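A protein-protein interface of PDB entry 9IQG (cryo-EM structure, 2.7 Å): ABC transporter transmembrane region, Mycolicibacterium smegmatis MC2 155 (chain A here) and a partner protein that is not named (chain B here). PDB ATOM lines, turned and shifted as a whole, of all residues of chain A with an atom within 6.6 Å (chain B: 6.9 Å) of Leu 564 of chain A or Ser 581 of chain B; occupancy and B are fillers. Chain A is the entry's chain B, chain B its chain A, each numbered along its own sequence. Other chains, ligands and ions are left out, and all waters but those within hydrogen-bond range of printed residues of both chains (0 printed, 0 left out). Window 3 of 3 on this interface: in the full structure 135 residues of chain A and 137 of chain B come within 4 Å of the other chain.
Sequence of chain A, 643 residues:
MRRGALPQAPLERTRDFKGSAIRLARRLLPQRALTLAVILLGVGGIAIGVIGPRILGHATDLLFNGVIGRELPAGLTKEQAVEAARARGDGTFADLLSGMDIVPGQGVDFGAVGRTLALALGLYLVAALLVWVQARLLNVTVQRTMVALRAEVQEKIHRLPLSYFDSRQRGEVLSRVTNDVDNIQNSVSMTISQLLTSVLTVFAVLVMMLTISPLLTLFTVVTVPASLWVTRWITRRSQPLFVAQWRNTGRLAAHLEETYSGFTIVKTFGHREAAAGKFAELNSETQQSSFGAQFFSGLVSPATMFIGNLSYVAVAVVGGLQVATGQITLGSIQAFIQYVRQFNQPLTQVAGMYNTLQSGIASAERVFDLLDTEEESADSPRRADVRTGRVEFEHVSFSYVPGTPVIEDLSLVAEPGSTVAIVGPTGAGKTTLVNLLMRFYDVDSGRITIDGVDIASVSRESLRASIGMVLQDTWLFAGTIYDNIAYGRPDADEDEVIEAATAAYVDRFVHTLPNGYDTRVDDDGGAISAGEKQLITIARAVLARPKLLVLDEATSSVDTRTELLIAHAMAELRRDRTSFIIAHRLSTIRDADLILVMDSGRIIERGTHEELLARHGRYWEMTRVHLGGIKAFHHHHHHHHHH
The backbone NH of Thr 562 of chain A is in hydrogen-bond range of the side-chain carboxylate of Asp 559 of chain A, 2.5 Å away.
The side-chain carboxylate of Asp 559 of chain A lies within hydrogen-bond range of the backbone NH of Arg 561 of chain A, 3.0 Å away.
The backbone NH (N) of Ile 542 of chain B lies within hydrogen-bond range of the side-chain amide oxygen (OE1) of Gln 582 of chain B.
The backbone carbonyl oxygen (O) of Phe 578 of chain B sits at hydrogen-bond distance from the side-chain hydroxyl (OG) of Ser 581 of chain B (2.7 Å).
Printed residues of chain B within 4 Å of Asp 559 of chain A: Phe 578 (3.8 Å).
Of the printed residues of chain B, Thr 560 of chain A touches Phe 578, Ser 581 and Gln 582.
Printed residues of chain A within 4 Å of Glu 577 of chain B: Arg 561.
Of the printed residues of chain A, Phe 578 of chain B touches Asp 559, Thr 560 and Arg 561.
Ser 581 of chain B touches just these residues of chain A: Thr 560 and Leu 564.
Of the printed residues of chain A, Gln 582 of chain B touches Thr 560.
The nearest residue of chain B that does not touch Leu 564 of chain A is Gln 582 of chain B (5.9 Å).
The nearest residue of chain A that does not touch Ser 581 of chain B is Arg 561 of chain A (4.02 Å).
The nearest printed residue of chain B that does not touch Asp 559 of chain A is Gln 582 of chain B (6.5 Å).
Along chain A the printed residues that touch a printed residue of chain B span positions 559 to 564.
OE1 of Glu 577 of chain B is in salt-bridge range of NE of Arg 561 of chain A (2.6 Å).
OG of Ser 581 of chain B sits at hydrogen-bond distance from OG1 of Thr 560 of chain A (2.5 Å).
Among the printed residues, merely in contact across the chains: Asp 559 of chain A with Phe 578 of chain B (3.8 Å), Thr 560 of chain A with Phe 578 of chain B (3.8 Å), Thr 560 of chain A with Gln 582 of chain B (3.3 Å), Arg 561 of chain A with Phe 578 of chain B (3.6 Å) and Leu 564 of chain A with Ser 581 of chain B (3.7 Å).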
ATOM      1  N   ASP A 559     -16.344  23.887 -23.630  1.00  0.00           N
ATOM      2  CA  ASP A 559     -15.749  22.649 -24.105  1.00  0.00           C
ATOM      3  C   ASP A 559     -14.888  22.898 -25.341  1.00  0.00           C
ATOM      4  O   ASP A 559     -15.009  23.917 -26.026  1.00  0.00           O
ATOM      5  CB  ASP A 559     -16.836  21.619 -24.413  1.00  0.00           C
ATOM      6  CG  ASP A 559     -17.726  22.036 -25.564  1.00  0.00           C
ATOM      7  OD1 ASP A 559     -17.360  21.780 -26.729  1.00  0.00           O
ATOM      8  OD2 ASP A 559     -18.797  22.621 -25.305  1.00  0.00           O
ATOM      9  N   THR A 560     -13.999  21.942 -25.617  1.00  0.00           N
ATOM     10  CA  THR A 560     -13.046  22.106 -26.710  1.00  0.00           C
ATOM     11  C   THR A 560     -13.733  22.053 -28.070  1.00  0.00           C
ATOM     12  O   THR A 560     -13.331  22.762 -28.999  1.00  0.00           O
ATOM     13  CB  THR A 560     -11.955  21.042 -26.618  1.00  0.00           C
ATOM     14  OG1 THR A 560     -12.452  19.798 -27.124  1.00  0.00           O
ATOM     15  CG2 THR A 560     -11.522  20.860 -25.174  1.00  0.00           C
ATOM     16  N   ARG A 561     -14.764  21.216 -28.209  1.00  0.00           N
ATOM     17  CA  ARG A 561     -15.481  21.140 -29.479  1.00  0.00           C
ATOM     18  C   ARG A 561     -16.153  22.465 -29.813  1.00  0.00           C
ATOM     19  O   ARG A 561     -16.130  22.908 -30.968  1.00  0.00           O
ATOM     20  CB  ARG A 561     -16.510  20.011 -29.437  1.00  0.00           C
ATOM     21  CG  ARG A 561     -15.902  18.622 -29.531  1.00  0.00           C
ATOM     22  CD  ARG A 561     -16.872  17.553 -29.059  1.00  0.00           C
ATOM     23  NE  ARG A 561     -18.060  17.469 -29.902  1.00  0.00           N
ATOM     24  CZ  ARG A 561     -19.300  17.651 -29.469  1.00  0.00           C
ATOM     25  NH1 ARG A 561     -19.555  17.940 -28.204  1.00  0.00           N
ATOM     26  NH2 ARG A 561     -20.309  17.539 -30.328  1.00  0.00           N
ATOM     27  N   THR A 562     -16.759  23.113 -28.817  1.00  0.00           N
ATOM     28  CA  THR A 562     -17.357  24.424 -29.042  1.00  0.00           C
ATOM     29  C   THR A 562     -16.287  25.495 -29.206  1.00  0.00           C
ATOM     30  O   THR A 562     -16.449  26.430 -30.002  1.00  0.00           O
ATOM     31  CB  THR A 562     -18.297  24.773 -27.889  1.00  0.00           C
ATOM     32  OG1 THR A 562     -19.213  23.693 -27.676  1.00  0.00           O
ATOM     33  CG2 THR A 562     -19.085  26.033 -28.199  1.00  0.00           C
ATOM     34  N   GLU A 563     -15.183  25.376 -28.465  1.00  0.00           N
ATOM     35  CA  GLU A 563     -14.140  26.393 -28.534  1.00  0.00           C
ATOM     36  C   GLU A 563     -13.427  26.378 -29.880  1.00  0.00           C
ATOM     37  O   GLU A 563     -12.941  27.421 -30.327  1.00  0.00           O
ATOM     38  CB  GLU A 563     -13.145  26.211 -27.387  1.00  0.00           C
ATOM     39  CG  GLU A 563     -11.808  25.612 -27.787  1.00  0.00           C
ATOM     40  CD  GLU A 563     -10.957  25.242 -26.589  1.00  0.00           C
ATOM     41  OE1 GLU A 563     -10.915  26.032 -25.622  1.00  0.00           O
ATOM     42  OE2 GLU A 563     -10.328  24.164 -26.614  1.00  0.00           O
ATOM     43  N   LEU A 564     -13.362  25.222 -30.546  1.00  0.00           N
ATOM     44  CA  LEU A 564     -12.779  25.183 -31.884  1.00  0.00           C
ATOM     45  C   LEU A 564     -13.613  25.993 -32.869  1.00  0.00           C
ATOM     46  O   LEU A 564     -13.076  26.783 -33.657  1.00  0.00           O
ATOM     47  CB  LEU A 564     -12.641  23.735 -32.356  1.00  0.00           C
ATOM     48  CG  LEU A 564     -11.401  22.983 -31.876  1.00  0.00           C
ATOM     49  CD1 LEU A 564     -11.463  21.528 -32.303  1.00  0.00           C
ATOM     50  CD2 LEU A 564     -10.141  23.645 -32.407  1.00  0.00           C
ATOM     51  N   LEU A 565     -14.935  25.818 -32.829  1.00  0.00           N
ATOM     52  CA  LEU A 565     -15.811  26.612 -33.683  1.00  0.00           C
ATOM     53  C   LEU A 565     -15.742  28.087 -33.314  1.00  0.00           C
ATOM     54  O   LEU A 565     -15.795  28.959 -34.190  1.00  0.00           O
ATOM     55  CB  LEU A 565     -17.245  26.096 -33.581  1.00  0.00           C
ATOM     56  CG  LEU A 565     -17.422  24.578 -33.617  1.00  0.00           C
ATOM     57  CD1 LEU A 565     -18.857  24.195 -33.302  1.00  0.00           C
ATOM     58  CD2 LEU A 565     -17.002  24.027 -34.970  1.00  0.00           C
ATOM     59  N   ILE A 566     -15.623  28.387 -32.019  1.00  0.00           N
ATOM     60  CA  ILE A 566     -15.495  29.774 -31.585  1.00  0.00           C
ATOM     61  C   ILE A 566     -14.227  30.395 -32.155  1.00  0.00           C
ATOM     62  O   ILE A 566     -14.238  31.536 -32.627  1.00  0.00           O
ATOM     63  CB  ILE A 566     -15.522  29.854 -30.049  1.00  0.00           C
ATOM     64  CG1 ILE A 566     -16.959  29.804 -29.544  1.00  0.00           C
ATOM     65  CG2 ILE A 566     -14.840  31.123 -29.562  1.00  0.00           C
ATOM     66  CD1 ILE A 566     -17.089  29.097 -28.232  1.00  0.00           C
ATOM     67  N   ALA A 567     -13.114  29.661 -32.111  1.00  0.00           N
ATOM     68  CA  ALA A 567     -11.864  30.166 -32.669  1.00  0.00           C
ATOM     69  C   ALA A 567     -11.969  30.350 -34.177  1.00  0.00           C
ATOM     70  O   ALA A 567     -11.452  31.331 -34.727  1.00  0.00           O
ATOM     71  CB  ALA A 567     -10.713  29.225 -32.319  1.00  0.00           C
ATOM     72  N   HIS A 568     -12.637  29.419 -34.862  1.00  0.00           N
ATOM     73  CA  HIS A 568     -12.837  29.571 -36.300  1.00  0.00           C
ATOM     74  C   HIS A 568     -13.635  30.833 -36.610  1.00  0.00           C
ATOM     75  O   HIS A 568     -13.310  31.568 -37.549  1.00  0.00           O
ATOM     76  CB  HIS A 568     -13.535  28.336 -36.867  1.00  0.00           C
ATOM     77  CG  HIS A 568     -13.556  28.281 -38.365  1.00  0.00           C
ATOM     78  ND1 HIS A 568     -14.094  29.284 -39.142  1.00  0.00           N
ATOM     79  CD2 HIS A 568     -13.104  27.340 -39.227  1.00  0.00           C
ATOM     80  CE1 HIS A 568     -13.971  28.964 -40.418  1.00  0.00           C
ATOM     81  NE2 HIS A 568     -13.374  27.789 -40.496  1.00  0.00           N
ATOM     82  N   ALA A 569     -14.684  31.099 -35.830  1.00  0.00           N
ATOM     83  CA  ALA A 569     -15.498  32.287 -36.067  1.00  0.00           C
ATOM     84  C   ALA A 569     -14.766  33.569 -35.686  1.00  0.00           C
ATOM     85  O   ALA A 569     -14.961  34.605 -36.331  1.00  0.00           O
ATOM     86  CB  ALA A 569     -16.815  32.182 -35.300  1.00  0.00           C
ATOM     87  N   SER A 587      -3.293  24.386 -26.489  1.00  0.00           N
ATOM     88  CA  SER A 587      -3.804  24.209 -27.843  1.00  0.00           C
ATOM     89  C   SER A 587      -4.472  25.476 -28.358  1.00  0.00           C
ATOM     90  O   SER A 587      -4.348  25.802 -29.544  1.00  0.00           O
ATOM     91  CB  SER A 587      -4.782  23.038 -27.886  1.00  0.00           C
ATOM     92  OG  SER A 587      -5.842  23.227 -26.966  1.00  0.00           O
ATOM     93  N   ILE B 542      -9.626  15.270 -21.957  1.00  0.00           N
ATOM     94  CA  ILE B 542      -9.691  13.816 -22.072  1.00  0.00           C
ATOM     95  C   ILE B 542      -8.473  13.167 -21.424  1.00  0.00           C
ATOM     96  O   ILE B 542      -8.563  12.054 -20.890  1.00  0.00           O
ATOM     97  CB  ILE B 542      -9.848  13.410 -23.553  1.00  0.00           C
ATOM     98  CG1 ILE B 542     -11.325  13.211 -23.919  1.00  0.00           C
ATOM     99  CG2 ILE B 542      -9.046  12.157 -23.883  1.00  0.00           C
ATOM    100  CD1 ILE B 542     -12.256  14.312 -23.461  1.00  0.00           C
ATOM    101  N   TYR B 575     -17.533  10.996 -27.779  1.00  0.00           N
ATOM    102  CA  TYR B 575     -16.244  10.877 -27.107  1.00  0.00           C
ATOM    103  C   TYR B 575     -15.100  10.854 -28.112  1.00  0.00           C
ATOM    104  O   TYR B 575     -14.036  11.434 -27.867  1.00  0.00           O
ATOM    105  CB  TYR B 575     -16.219   9.622 -26.237  1.00  0.00           C
ATOM    106  CG  TYR B 575     -15.043   9.561 -25.294  1.00  0.00           C
ATOM    107  CD1 TYR B 575     -15.092  10.175 -24.050  1.00  0.00           C
ATOM    108  CD2 TYR B 575     -13.881   8.892 -25.650  1.00  0.00           C
ATOM    109  CE1 TYR B 575     -14.018  10.122 -23.186  1.00  0.00           C
ATOM    110  CE2 TYR B 575     -12.803   8.834 -24.793  1.00  0.00           C
ATOM    111  CZ  TYR B 575     -12.876   9.450 -23.563  1.00  0.00           C
ATOM    112  OH  TYR B 575     -11.802   9.393 -22.707  1.00  0.00           O
ATOM    113  N   ALA B 576     -15.301  10.180 -29.247  1.00  0.00           N
ATOM    114  CA  ALA B 576     -14.286  10.178 -30.293  1.00  0.00           C
ATOM    115  C   ALA B 576     -14.054  11.583 -30.835  1.00  0.00           C
ATOM    116  O   ALA B 576     -12.912  11.978 -31.085  1.00  0.00           O
ATOM    117  CB  ALA B 576     -14.691   9.227 -31.417  1.00  0.00           C
ATOM    118  N   GLU B 577     -15.130  12.351 -31.023  1.00  0.00           N
ATOM    119  CA  GLU B 577     -14.983  13.730 -31.478  1.00  0.00           C
ATOM    120  C   GLU B 577     -14.236  14.574 -30.452  1.00  0.00           C
ATOM    121  O   GLU B 577     -13.384  15.393 -30.815  1.00  0.00           O
ATOM    122  CB  GLU B 577     -16.355  14.335 -31.773  1.00  0.00           C
ATOM    123  CG  GLU B 577     -16.296  15.683 -32.471  1.00  0.00           C
ATOM    124  CD  GLU B 577     -17.634  16.101 -33.043  1.00  0.00           C
ATOM    125  OE1 GLU B 577     -18.558  16.386 -32.252  1.00  0.00           O
ATOM    126  OE2 GLU B 577     -17.763  16.144 -34.284  1.00  0.00           O
ATOM    127  N   PHE B 578     -14.544  14.389 -29.167  1.00  0.00           N
ATOM    128  CA  PHE B 578     -13.833  15.120 -28.121  1.00  0.00           C
ATOM    129  C   PHE B 578     -12.346  14.782 -28.123  1.00  0.00           C
ATOM    130  O   PHE B 578     -11.493  15.676 -28.029  1.00  0.00           O
ATOM    131  CB  PHE B 578     -14.447  14.809 -26.755  1.00  0.00           C
ATOM    132  CG  PHE B 578     -15.358  15.884 -26.238  1.00  0.00           C
ATOM    133  CD1 PHE B 578     -16.706  15.633 -26.041  1.00  0.00           C
ATOM    134  CD2 PHE B 578     -14.867  17.145 -25.948  1.00  0.00           C
ATOM    135  CE1 PHE B 578     -17.547  16.620 -25.565  1.00  0.00           C
ATOM    136  CE2 PHE B 578     -15.704  18.137 -25.471  1.00  0.00           C
ATOM    137  CZ  PHE B 578     -17.044  17.873 -25.280  1.00  0.00           C
ATOM    138  N   ALA B 579     -12.019  13.492 -28.237  1.00  0.00           N
ATOM    139  CA  ALA B 579     -10.620  13.078 -28.263  1.00  0.00           C
ATOM    140  C   ALA B 579      -9.905  13.616 -29.495  1.00  0.00           C
ATOM    141  O   ALA B 579      -8.750  14.049 -29.411  1.00  0.00           O
ATOM    142  CB  ALA B 579     -10.523  11.554 -28.207  1.00  0.00           C
ATOM    143  N   GLU B 580     -10.571  13.596 -30.650  1.00  0.00           N
ATOM    144  CA  GLU B 580      -9.972  14.147 -31.861  1.00  0.00           C
ATOM    145  C   GLU B 580      -9.728  15.644 -31.723  1.00  0.00           C
ATOM    146  O   GLU B 580      -8.688  16.155 -32.154  1.00  0.00           O
ATOM    147  CB  GLU B 580     -10.864  13.851 -33.067  1.00  0.00           C
ATOM    148  CG  GLU B 580     -10.662  14.791 -34.244  1.00  0.00           C
ATOM    149  CD  GLU B 580     -11.313  14.280 -35.512  1.00  0.00           C
ATOM    150  OE1 GLU B 580     -11.649  13.079 -35.566  1.00  0.00           O
ATOM    151  OE2 GLU B 580     -11.489  15.080 -36.455  1.00  0.00           O
ATOM    152  N   SER B 581     -10.678  16.363 -31.122  1.00  0.00           N
ATOM    153  CA  SER B 581     -10.508  17.799 -30.928  1.00  0.00           C
ATOM    154  C   SER B 581      -9.350  18.096 -29.985  1.00  0.00           C
ATOM    155  O   SER B 581      -8.590  19.047 -30.204  1.00  0.00           O
ATOM    156  CB  SER B 581     -11.803  18.414 -30.398  1.00  0.00           C
ATOM    157  OG  SER B 581     -11.939  18.194 -29.005  1.00  0.00           O
ATOM    158  N   GLN B 582      -9.198  17.298 -28.932  1.00  0.00           N
ATOM    159  CA  GLN B 582      -8.153  17.539 -27.945  1.00  0.00           C
ATOM    160  C   GLN B 582      -6.811  16.919 -28.317  1.00  0.00           C
ATOM    161  O   GLN B 582      -5.822  17.163 -27.618  1.00  0.00           O
ATOM    162  CB  GLN B 582      -8.592  17.020 -26.577  1.00  0.00           C
ATOM    163  CG  GLN B 582      -9.777  17.761 -26.002  1.00  0.00           C
ATOM    164  CD  GLN B 582     -10.093  17.333 -24.592  1.00  0.00           C
ATOM    165  OE1 GLN B 582      -9.287  16.673 -23.937  1.00  0.00           O
ATOM    166  NE2 GLN B 582     -11.273  17.699 -24.113  1.00  0.00           N
ATOM    167  N   ALA B 583      -6.755  16.121 -29.381  1.00  0.00           N
ATOM    168  CA  ALA B 583      -5.494  15.525 -29.799  1.00  0.00           C
ATOM    169  C   ALA B 583      -4.482  16.598 -30.178  1.00  0.00           C
ATOM    170  O   ALA B 583      -4.828  17.623 -30.772  1.00  0.00           O
ATOM    171  CB  ALA B 583      -5.723  14.577 -30.976  1.00  0.00           C
ATOM    172  N   LEU B 584      -3.224  16.356 -29.828  1.00  0.00           N
ATOM    173  CA  LEU B 584      -2.152  17.307 -30.099  1.00  0.00           C
ATOM    174  C   LEU B 584      -1.262  16.820 -31.239  1.00  0.00           C
ATOM    175  O   LEU B 584      -0.502  15.863 -31.081  1.00  0.00           O
ATOM    176  CB  LEU B 584      -1.315  17.541 -28.840  1.00  0.00           C
ATOM    177  CG  LEU B 584      -0.093  18.448 -28.987  1.00  0.00           C
ATOM    178  CD1 LEU B 584      -0.511  19.836 -29.445  1.00  0.00           C
ATOM    179  CD2 LEU B 584       0.683  18.521 -27.682  1.00  0.00           C
